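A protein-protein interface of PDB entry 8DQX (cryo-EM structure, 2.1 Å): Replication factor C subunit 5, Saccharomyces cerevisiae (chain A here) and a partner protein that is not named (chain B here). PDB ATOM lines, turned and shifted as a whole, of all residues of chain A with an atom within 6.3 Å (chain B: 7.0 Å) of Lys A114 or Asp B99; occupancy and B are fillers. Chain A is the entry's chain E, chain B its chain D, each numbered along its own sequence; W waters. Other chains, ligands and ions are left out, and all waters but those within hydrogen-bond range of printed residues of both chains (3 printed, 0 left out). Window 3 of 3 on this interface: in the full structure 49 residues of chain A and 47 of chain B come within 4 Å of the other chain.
O of Ala B97 is in hydrogen-bond range of NE2 of Gln A110 (3.0 Å).
The backbone carbonyl oxygen of Ser B98 lies close to the side-chain amide nitrogen of Gln A110.
OG of Ser B98 lies within hydrogen-bond range of NZ of Lys A114 (3.0 Å).
O of Asp B99 lies within hydrogen-bond range of NE2 of Gln A110 (3.3 Å).
The side-chain amino group (NZ) of Lys A114 lies within salt-bridge range of the side-chain carboxylate (OD1) of Asp B99 (2.6 Å).
Of the printed residues of chain B, Gln A110 touches Ala B97, Ser B98 and Asp B99.
Printed residues of chain B within 4 Å of Lys A114: Ser B98 and Asp B99.
Printed residues of chain B within 4 Å of Lys A160: Asn B96 (3.8 Å).
Of the printed residues of chain A, Asn B96 touches Lys A160.
Asp B99 touches just these residues of chain A: Gln A110 (3.3 Å) and Lys A114 (2.6 Å).
The nearest residue of chain A that does not touch Asp B99 is Ala A153 (6.1 Å).
The nearest printed residue of chain A that does not touch Asn B96 is Lys A114 (5.0 Å).
Of the 17 printed residues of chain A, 4 touch a printed residue of chain B.
Along chain A the printed residues that touch a printed residue of chain B span positions 110 to 160.
Among the printed residues, 8 pairs touch across the chains.
Among the printed residues, Asp or Glu carboxylates within 4 Å of a Lys or Arg side-chain nitrogen of the other chain: Lys A114 with Asp B99 (2.6 Å).
The side-chain amide nitrogen of Asn B96 sits at hydrogen-bond distance from the side-chain carboxylate of Glu B94, at 2.9 Å.
OD1 of Asn B96 is in hydrogen-bond range of OG of Ser B98 (2.5 Å).
The backbone NH (N) of Asn B96 sits at hydrogen-bond distance from the side-chain carboxylate (OD2) of Asp B99.
The backbone carbonyl oxygen (O) of Asn B96 lies within hydrogen-bond range of the guanidinium group (NE) of Arg B101, at 3.3 Å.
The backbone NH (N) of Lys A114 lies within hydrogen-bond range of the backbone carbonyl oxygen (O) of Ile A109.
Among the printed residues, pairs that only touch across the chains: Ala A153 with Ala B97 (3.7 Å), Ala A153 with Ser B98 (3.5 Å) and Lys A160 with Asn B96 (3.8 Å).
Water W2 bridges the side-chain hydroxyl of Ser B98 (2.8 Å) and the side-chain hydroxyl of Thr A157 (2.8 Å).
Water W1 bridges the guanidinium group of Arg A106 (3.0 Å) and the backbone carbonyl oxygen of Ala B97 (3.2 Å).
Water W3 lies within hydrogen-bond range of N of Ser B98 (3.3 Å), OD1 of Asn B96 (3.5 Å) and O of Ala A153 (3.5 Å).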
ATOM      1  N   ARG A 106       3.119  27.932   8.688  1.00  0.00           N
ATOM      2  CA  ARG A 106       3.932  28.124   7.494  1.00  0.00           C
ATOM      3  C   ARG A 106       4.623  26.830   7.079  1.00  0.00           C
ATOM      4  O   ARG A 106       4.665  26.494   5.891  1.00  0.00           O
ATOM      5  CB  ARG A 106       4.960  29.226   7.737  1.00  0.00           C
ATOM      6  CG  ARG A 106       5.603  29.745   6.468  1.00  0.00           C
ATOM      7  CD  ARG A 106       7.113  29.711   6.569  1.00  0.00           C
ATOM      8  NE  ARG A 106       7.606  30.574   7.636  1.00  0.00           N
ATOM      9  CZ  ARG A 106       8.010  31.827   7.473  1.00  0.00           C
ATOM     10  NH1 ARG A 106       8.005  32.411   6.286  1.00  0.00           N
ATOM     11  NH2 ARG A 106       8.429  32.514   8.532  1.00  0.00           N
ATOM     12  N   VAL A 108       3.603  23.821   7.382  1.00  0.00           N
ATOM     13  CA  VAL A 108       2.630  22.978   6.696  1.00  0.00           C
ATOM     14  C   VAL A 108       2.523  23.385   5.234  1.00  0.00           C
ATOM     15  O   VAL A 108       2.433  22.534   4.343  1.00  0.00           O
ATOM     16  CB  VAL A 108       1.265  23.051   7.407  1.00  0.00           C
ATOM     17  CG1 VAL A 108       0.215  22.262   6.635  1.00  0.00           C
ATOM     18  CG2 VAL A 108       1.379  22.543   8.838  1.00  0.00           C
ATOM     19  N   ILE A 109       2.526  24.690   4.961  1.00  0.00           N
ATOM     20  CA  ILE A 109       2.418  25.132   3.577  1.00  0.00           C
ATOM     21  C   ILE A 109       3.701  24.821   2.817  1.00  0.00           C
ATOM     22  O   ILE A 109       3.659  24.359   1.671  1.00  0.00           O
ATOM     23  CB  ILE A 109       2.066  26.629   3.509  1.00  0.00           C
ATOM     24  CG1 ILE A 109       0.824  26.933   4.355  1.00  0.00           C
ATOM     25  CG2 ILE A 109       1.837  27.045   2.068  1.00  0.00           C
ATOM     26  CD1 ILE A 109      -0.360  26.074   4.031  1.00  0.00           C
ATOM     27  N   GLN A 110       4.858  25.040   3.446  1.00  0.00           N
ATOM     28  CA  GLN A 110       6.111  24.966   2.706  1.00  0.00           C
ATOM     29  C   GLN A 110       6.557  23.535   2.436  1.00  0.00           C
ATOM     30  O   GLN A 110       7.300  23.311   1.475  1.00  0.00           O
ATOM     31  CB  GLN A 110       7.213  25.728   3.453  1.00  0.00           C
ATOM     32  CG  GLN A 110       7.125  27.245   3.274  1.00  0.00           C
ATOM     33  CD  GLN A 110       8.241  28.001   3.973  1.00  0.00           C
ATOM     34  OE1 GLN A 110       8.640  27.655   5.081  1.00  0.00           O
ATOM     35  NE2 GLN A 110       8.740  29.049   3.329  1.00  0.00           N
ATOM     36  N   GLU A 111       6.117  22.564   3.236  1.00  0.00           N
ATOM     37  CA  GLU A 111       6.564  21.184   3.095  1.00  0.00           C
ATOM     38  C   GLU A 111       5.449  20.251   2.641  1.00  0.00           C
ATOM     39  O   GLU A 111       5.576  19.606   1.598  1.00  0.00           O
ATOM     40  CB  GLU A 111       7.160  20.691   4.419  1.00  0.00           C
ATOM     41  CG  GLU A 111       8.379  21.478   4.859  1.00  0.00           C
ATOM     42  CD  GLU A 111       8.851  21.102   6.247  1.00  0.00           C
ATOM     43  OE1 GLU A 111       8.247  20.197   6.860  1.00  0.00           O
ATOM     44  OE2 GLU A 111       9.832  21.709   6.724  1.00  0.00           O
ATOM     45  N   LEU A 112       4.347  20.170   3.389  1.00  0.00           N
ATOM     46  CA  LEU A 112       3.283  19.239   3.029  1.00  0.00           C
ATOM     47  C   LEU A 112       2.628  19.645   1.713  1.00  0.00           C
ATOM     48  O   LEU A 112       2.681  18.902   0.727  1.00  0.00           O
ATOM     49  CB  LEU A 112       2.254  19.162   4.160  1.00  0.00           C
ATOM     50  CG  LEU A 112       0.927  18.456   3.854  1.00  0.00           C
ATOM     51  CD1 LEU A 112       0.376  17.769   5.096  1.00  0.00           C
ATOM     52  CD2 LEU A 112      -0.105  19.420   3.292  1.00  0.00           C
ATOM     53  N   LEU A 113       2.033  20.838   1.666  1.00  0.00           N
ATOM     54  CA  LEU A 113       1.326  21.248   0.457  1.00  0.00           C
ATOM     55  C   LEU A 113       2.235  21.176  -0.763  1.00  0.00           C
ATOM     56  O   LEU A 113       1.886  20.544  -1.769  1.00  0.00           O
ATOM     57  CB  LEU A 113       0.764  22.658   0.630  1.00  0.00           C
ATOM     58  CG  LEU A 113      -0.212  23.132  -0.452  1.00  0.00           C
ATOM     59  CD1 LEU A 113      -1.321  22.112  -0.692  1.00  0.00           C
ATOM     60  CD2 LEU A 113      -0.793  24.477  -0.081  1.00  0.00           C
ATOM     61  N   LYS A 114       3.426  21.771  -0.671  1.00  0.00           N
ATOM     62  CA  LYS A 114       4.366  21.718  -1.783  1.00  0.00           C
ATOM     63  C   LYS A 114       4.581  20.286  -2.252  1.00  0.00           C
ATOM     64  O   LYS A 114       4.563  20.012  -3.458  1.00  0.00           O
ATOM     65  CB  LYS A 114       5.695  22.354  -1.377  1.00  0.00           C
ATOM     66  CG  LYS A 114       6.554  22.788  -2.554  1.00  0.00           C
ATOM     67  CD  LYS A 114       7.438  23.972  -2.194  1.00  0.00           C
ATOM     68  CE  LYS A 114       8.194  24.496  -3.399  1.00  0.00           C
ATOM     69  NZ  LYS A 114       9.268  25.448  -3.008  1.00  0.00           N
ATOM     70  N   GLU A 115       4.763  19.352  -1.318  1.00  0.00           N
ATOM     71  CA  GLU A 115       4.989  17.967  -1.717  1.00  0.00           C
ATOM     72  C   GLU A 115       3.812  17.439  -2.525  1.00  0.00           C
ATOM     73  O   GLU A 115       4.001  16.861  -3.604  1.00  0.00           O
ATOM     74  CB  GLU A 115       5.243  17.099  -0.484  1.00  0.00           C
ATOM     75  CG  GLU A 115       5.028  15.606  -0.696  1.00  0.00           C
ATOM     76  CD  GLU A 115       3.571  15.188  -0.578  1.00  0.00           C
ATOM     77  OE1 GLU A 115       2.791  15.922   0.065  1.00  0.00           O
ATOM     78  OE2 GLU A 115       3.207  14.131  -1.138  1.00  0.00           O
ATOM     79  N   VAL A 116       2.586  17.668  -2.049  1.00  0.00           N
ATOM     80  CA  VAL A 116       1.426  17.191  -2.794  1.00  0.00           C
ATOM     81  C   VAL A 116       1.453  17.767  -4.201  1.00  0.00           C
ATOM     82  O   VAL A 116       1.064  17.105  -5.170  1.00  0.00           O
ATOM     83  CB  VAL A 116       0.119  17.551  -2.064  1.00  0.00           C
ATOM     84  CG1 VAL A 116      -1.074  17.344  -2.991  1.00  0.00           C
ATOM     85  CG2 VAL A 116      -0.037  16.727  -0.805  1.00  0.00           C
ATOM     86  N   ALA A 117       1.940  19.000  -4.336  1.00  0.00           N
ATOM     87  CA  ALA A 117       1.932  19.663  -5.633  1.00  0.00           C
ATOM     88  C   ALA A 117       2.932  19.030  -6.594  1.00  0.00           C
ATOM     89  O   ALA A 117       2.711  19.030  -7.808  1.00  0.00           O
ATOM     90  CB  ALA A 117       2.227  21.150  -5.460  1.00  0.00           C
ATOM     91  N   GLN A 118       4.042  18.495  -6.081  1.00  0.00           N
ATOM     92  CA  GLN A 118       5.130  18.051  -6.949  1.00  0.00           C
ATOM     93  C   GLN A 118       5.060  16.574  -7.313  1.00  0.00           C
ATOM     94  O   GLN A 118       5.889  16.110  -8.101  1.00  0.00           O
ATOM     95  CB  GLN A 118       6.484  18.343  -6.291  1.00  0.00           C
ATOM     96  CG  GLN A 118       6.747  19.819  -6.051  1.00  0.00           C
ATOM     97  CD  GLN A 118       7.940  20.077  -5.146  1.00  0.00           C
ATOM     98  OE1 GLN A 118       8.777  20.928  -5.440  1.00  0.00           O
ATOM     99  NE2 GLN A 118       8.019  19.349  -4.036  1.00  0.00           N
ATOM    100  N   MET A 119       4.102  15.825  -6.779  1.00  0.00           N
ATOM    101  CA  MET A 119       4.063  14.382  -6.951  1.00  0.00           C
ATOM    102  C   MET A 119       2.831  13.956  -7.736  1.00  0.00           C
ATOM    103  O   MET A 119       1.765  14.569  -7.639  1.00  0.00           O
ATOM    104  CB  MET A 119       4.071  13.664  -5.597  1.00  0.00           C
ATOM    105  CG  MET A 119       5.412  13.712  -4.886  1.00  0.00           C
ATOM    106  SD  MET A 119       6.735  12.777  -5.694  1.00  0.00           S
ATOM    107  CE  MET A 119       5.848  11.419  -6.453  1.00  0.00           C
ATOM    108  N   ALA A 153       3.630  31.887   1.454  1.00  0.00           N
ATOM    109  CA  ALA A 153       4.158  30.615   0.973  1.00  0.00           C
ATOM    110  C   ALA A 153       3.223  29.947  -0.026  1.00  0.00           C
ATOM    111  O   ALA A 153       3.678  29.122  -0.824  1.00  0.00           O
ATOM    112  CB  ALA A 153       4.425  29.675   2.151  1.00  0.00           C
ATOM    113  N   THR A 157       3.267  28.431  -5.258  1.00  0.00           N
ATOM    114  CA  THR A 157       2.772  27.069  -5.416  1.00  0.00           C
ATOM    115  C   THR A 157       1.476  27.059  -6.219  1.00  0.00           C
ATOM    116  O   THR A 157       1.279  26.196  -7.080  1.00  0.00           O
ATOM    117  CB  THR A 157       2.574  26.412  -4.047  1.00  0.00           C
ATOM    118  OG1 THR A 157       3.851  26.116  -3.469  1.00  0.00           O
ATOM    119  CG2 THR A 157       1.778  25.122  -4.173  1.00  0.00           C
ATOM    120  N   LYS A 160       2.827  27.863 -10.109  1.00  0.00           N
ATOM    121  CA  LYS A 160       3.783  26.985 -10.773  1.00  0.00           C
ATOM    122  C   LYS A 160       3.182  25.612 -11.061  1.00  0.00           C
ATOM    123  O   LYS A 160       3.397  25.050 -12.138  1.00  0.00           O
ATOM    124  CB  LYS A 160       5.035  26.857  -9.907  1.00  0.00           C
ATOM    125  CG  LYS A 160       6.321  26.660 -10.685  1.00  0.00           C
ATOM    126  CD  LYS A 160       7.544  26.462  -9.778  1.00  0.00           C
ATOM    127  CE  LYS A 160       7.532  27.342  -8.526  1.00  0.00           C
ATOM    128  NZ  LYS A 160       7.515  28.800  -8.842  1.00  0.00           N
ATOM    129  N   TYR A 161       2.424  25.061 -10.115  1.00  0.00           N
ATOM    130  CA  TYR A 161       1.950  23.684 -10.202  1.00  0.00           C
ATOM    131  C   TYR A 161       0.453  23.598 -10.491  1.00  0.00           C
ATOM    132  O   TYR A 161      -0.184  22.595 -10.172  1.00  0.00           O
ATOM    133  CB  TYR A 161       2.280  22.932  -8.917  1.00  0.00           C
ATOM    134  CG  TYR A 161       3.751  22.912  -8.604  1.00  0.00           C
ATOM    135  CD1 TYR A 161       4.606  22.042  -9.263  1.00  0.00           C
ATOM    136  CD2 TYR A 161       4.287  23.759  -7.644  1.00  0.00           C
ATOM    137  CE1 TYR A 161       5.953  22.022  -8.982  1.00  0.00           C
ATOM    138  CE2 TYR A 161       5.633  23.741  -7.353  1.00  0.00           C
ATOM    139  CZ  TYR A 161       6.461  22.872  -8.025  1.00  0.00           C
ATOM    140  OH  TYR A 161       7.803  22.852  -7.735  1.00  0.00           O
ATOM    141  N   GLU B  94      15.965  30.405  -8.638  1.00  0.00           N
ATOM    142  CA  GLU B  94      14.724  31.050  -8.225  1.00  0.00           C
ATOM    143  C   GLU B  94      14.373  30.633  -6.803  1.00  0.00           C
ATOM    144  O   GLU B  94      14.251  29.440  -6.511  1.00  0.00           O
ATOM    145  CB  GLU B  94      13.587  30.698  -9.185  1.00  0.00           C
ATOM    146  CG  GLU B  94      12.419  31.680  -9.197  1.00  0.00           C
ATOM    147  CD  GLU B  94      11.891  32.002  -7.814  1.00  0.00           C
ATOM    148  OE1 GLU B  94      11.329  31.094  -7.170  1.00  0.00           O
ATOM    149  OE2 GLU B  94      12.032  33.161  -7.371  1.00  0.00           O
ATOM    150  N   LEU B  95      14.202  31.618  -5.928  1.00  0.00           N
ATOM    151  CA  LEU B  95      13.803  31.392  -4.547  1.00  0.00           C
ATOM    152  C   LEU B  95      12.676  32.356  -4.211  1.00  0.00           C
ATOM    153  O   LEU B  95      12.812  33.565  -4.415  1.00  0.00           O
ATOM    154  CB  LEU B  95      14.986  31.591  -3.591  1.00  0.00           C
ATOM    155  CG  LEU B  95      16.121  30.566  -3.674  1.00  0.00           C
ATOM    156  CD1 LEU B  95      17.238  30.938  -2.720  1.00  0.00           C
ATOM    157  CD2 LEU B  95      15.618  29.156  -3.379  1.00  0.00           C
ATOM    158  N   ASN B  96      11.573  31.825  -3.691  1.00  0.00           N
ATOM    159  CA  ASN B  96      10.377  32.618  -3.442  1.00  0.00           C
ATOM    160  C   ASN B  96       9.896  32.338  -2.023  1.00  0.00           C
ATOM    161  O   ASN B  96      10.561  31.653  -1.241  1.00  0.00           O
ATOM    162  CB  ASN B  96       9.307  32.310  -4.499  1.00  0.00           C
ATOM    163  CG  ASN B  96       8.891  30.857  -4.491  1.00  0.00           C
ATOM    164  OD1 ASN B  96       8.415  30.347  -3.481  1.00  0.00           O
ATOM    165  ND2 ASN B  96       9.093  30.174  -5.612  1.00  0.00           N
ATOM    166  N   ALA B  97       8.714  32.868  -1.693  1.00  0.00           N
ATOM    167  CA  ALA B  97       8.201  32.768  -0.332  1.00  0.00           C
ATOM    168  C   ALA B  97       7.898  31.331   0.079  1.00  0.00           C
ATOM    169  O   ALA B  97       7.775  31.062   1.277  1.00  0.00           O
ATOM    170  CB  ALA B  97       6.944  33.627  -0.181  1.00  0.00           C
ATOM    171  N   SER B  98       7.764  30.409  -0.873  1.00  0.00           N
ATOM    172  CA  SER B  98       7.547  29.007  -0.531  1.00  0.00           C
ATOM    173  C   SER B  98       8.825  28.304  -0.089  1.00  0.00           C
ATOM    174  O   SER B  98       8.745  27.197   0.449  1.00  0.00           O
ATOM    175  CB  SER B  98       6.936  28.257  -1.719  1.00  0.00           C
ATOM    176  OG  SER B  98       7.891  28.047  -2.744  1.00  0.00           O
ATOM    177  N   ASP B  99       9.987  28.917  -0.294  1.00  0.00           N
ATOM    178  CA  ASP B  99      11.273  28.330   0.053  1.00  0.00           C
ATOM    179  C   ASP B  99      11.800  28.918   1.357  1.00  0.00           C
ATOM    180  O   ASP B  99      11.461  30.038   1.738  1.00  0.00           O
ATOM    181  CB  ASP B  99      12.289  28.566  -1.068  1.00  0.00           C
ATOM    182  CG  ASP B  99      11.811  28.036  -2.408  1.00  0.00           C
ATOM    183  OD1 ASP B  99      11.404  26.858  -2.468  1.00  0.00           O
ATOM    184  OD2 ASP B  99      11.833  28.792  -3.400  1.00  0.00           O
ATOM    185  N   GLU B 100      12.653  28.150   2.033  1.00  0.00           N
ATOM    186  CA  GLU B 100      13.301  28.615   3.252  1.00  0.00           C
ATOM    187  C   GLU B 100      14.415  29.592   2.883  1.00  0.00           C
ATOM    188  O   GLU B 100      15.299  29.256   2.091  1.00  0.00           O
ATOM    189  CB  GLU B 100      13.844  27.423   4.040  1.00  0.00           C
ATOM    190  CG  GLU B 100      14.912  27.770   5.051  1.00  0.00           C
ATOM    191  CD  GLU B 100      14.394  28.671   6.144  1.00  0.00           C
ATOM    192  OE1 GLU B 100      13.182  28.593   6.446  1.00  0.00           O
ATOM    193  OE2 GLU B 100      15.191  29.458   6.697  1.00  0.00           O
ATOM    194  N   ARG B 101      14.381  30.794   3.457  1.00  0.00           N
ATOM    195  CA  ARG B 101      15.301  31.854   3.051  1.00  0.00           C
ATOM    196  C   ARG B 101      15.872  32.584   4.260  1.00  0.00           C
ATOM    197  O   ARG B 101      16.066  33.802   4.233  1.00  0.00           O
ATOM    198  CB  ARG B 101      14.617  32.842   2.108  1.00  0.00           C
ATOM    199  CG  ARG B 101      14.091  32.203   0.840  1.00  0.00           C
ATOM    200  CD  ARG B 101      13.569  33.231  -0.137  1.00  0.00           C
ATOM    201  NE  ARG B 101      12.399  33.927   0.378  1.00  0.00           N
ATOM    202  CZ  ARG B 101      11.729  34.859  -0.286  1.00  0.00           C
ATOM    203  NH1 ARG B 101      12.070  35.213  -1.516  1.00  0.00           N
ATOM    204  NH2 ARG B 101      10.682  35.439   0.291  1.00  0.00           N
ATOM    205  N   GLY B 102      16.176  31.853   5.326  1.00  0.00           N
ATOM    206  CA  GLY B 102      16.788  32.451   6.491  1.00  0.00           C
ATOM    207  C   GLY B 102      18.219  32.889   6.218  1.00  0.00           C
ATOM    208  O   GLY B 102      18.784  32.685   5.145  1.00  0.00           O
ATOM    209  N   ILE B 105      20.573  30.271   4.912  1.00  0.00           N
ATOM    210  CA  ILE B 105      20.390  30.002   3.487  1.00  0.00           C
ATOM    211  C   ILE B 105      21.082  31.070   2.648  1.00  0.00           C
ATOM    212  O   ILE B 105      21.812  30.755   1.704  1.00  0.00           O
ATOM    213  CB  ILE B 105      18.891  29.911   3.138  1.00  0.00           C
ATOM    214  CG1 ILE B 105      18.253  28.680   3.784  1.00  0.00           C
ATOM    215  CG2 ILE B 105      18.683  29.902   1.618  1.00  0.00           C
ATOM    216  CD1 ILE B 105      18.782  27.361   3.293  1.00  0.00           C
HETATM  217  O   HOH W   1       6.414  32.484   3.763  1.00  0.00           O
HETATM  218  O   HOH W   2       6.253  26.875  -4.644  1.00  0.00           O
HETATM  219  O   HOH W   3       5.273  31.562  -2.735  1.00  0.00           O
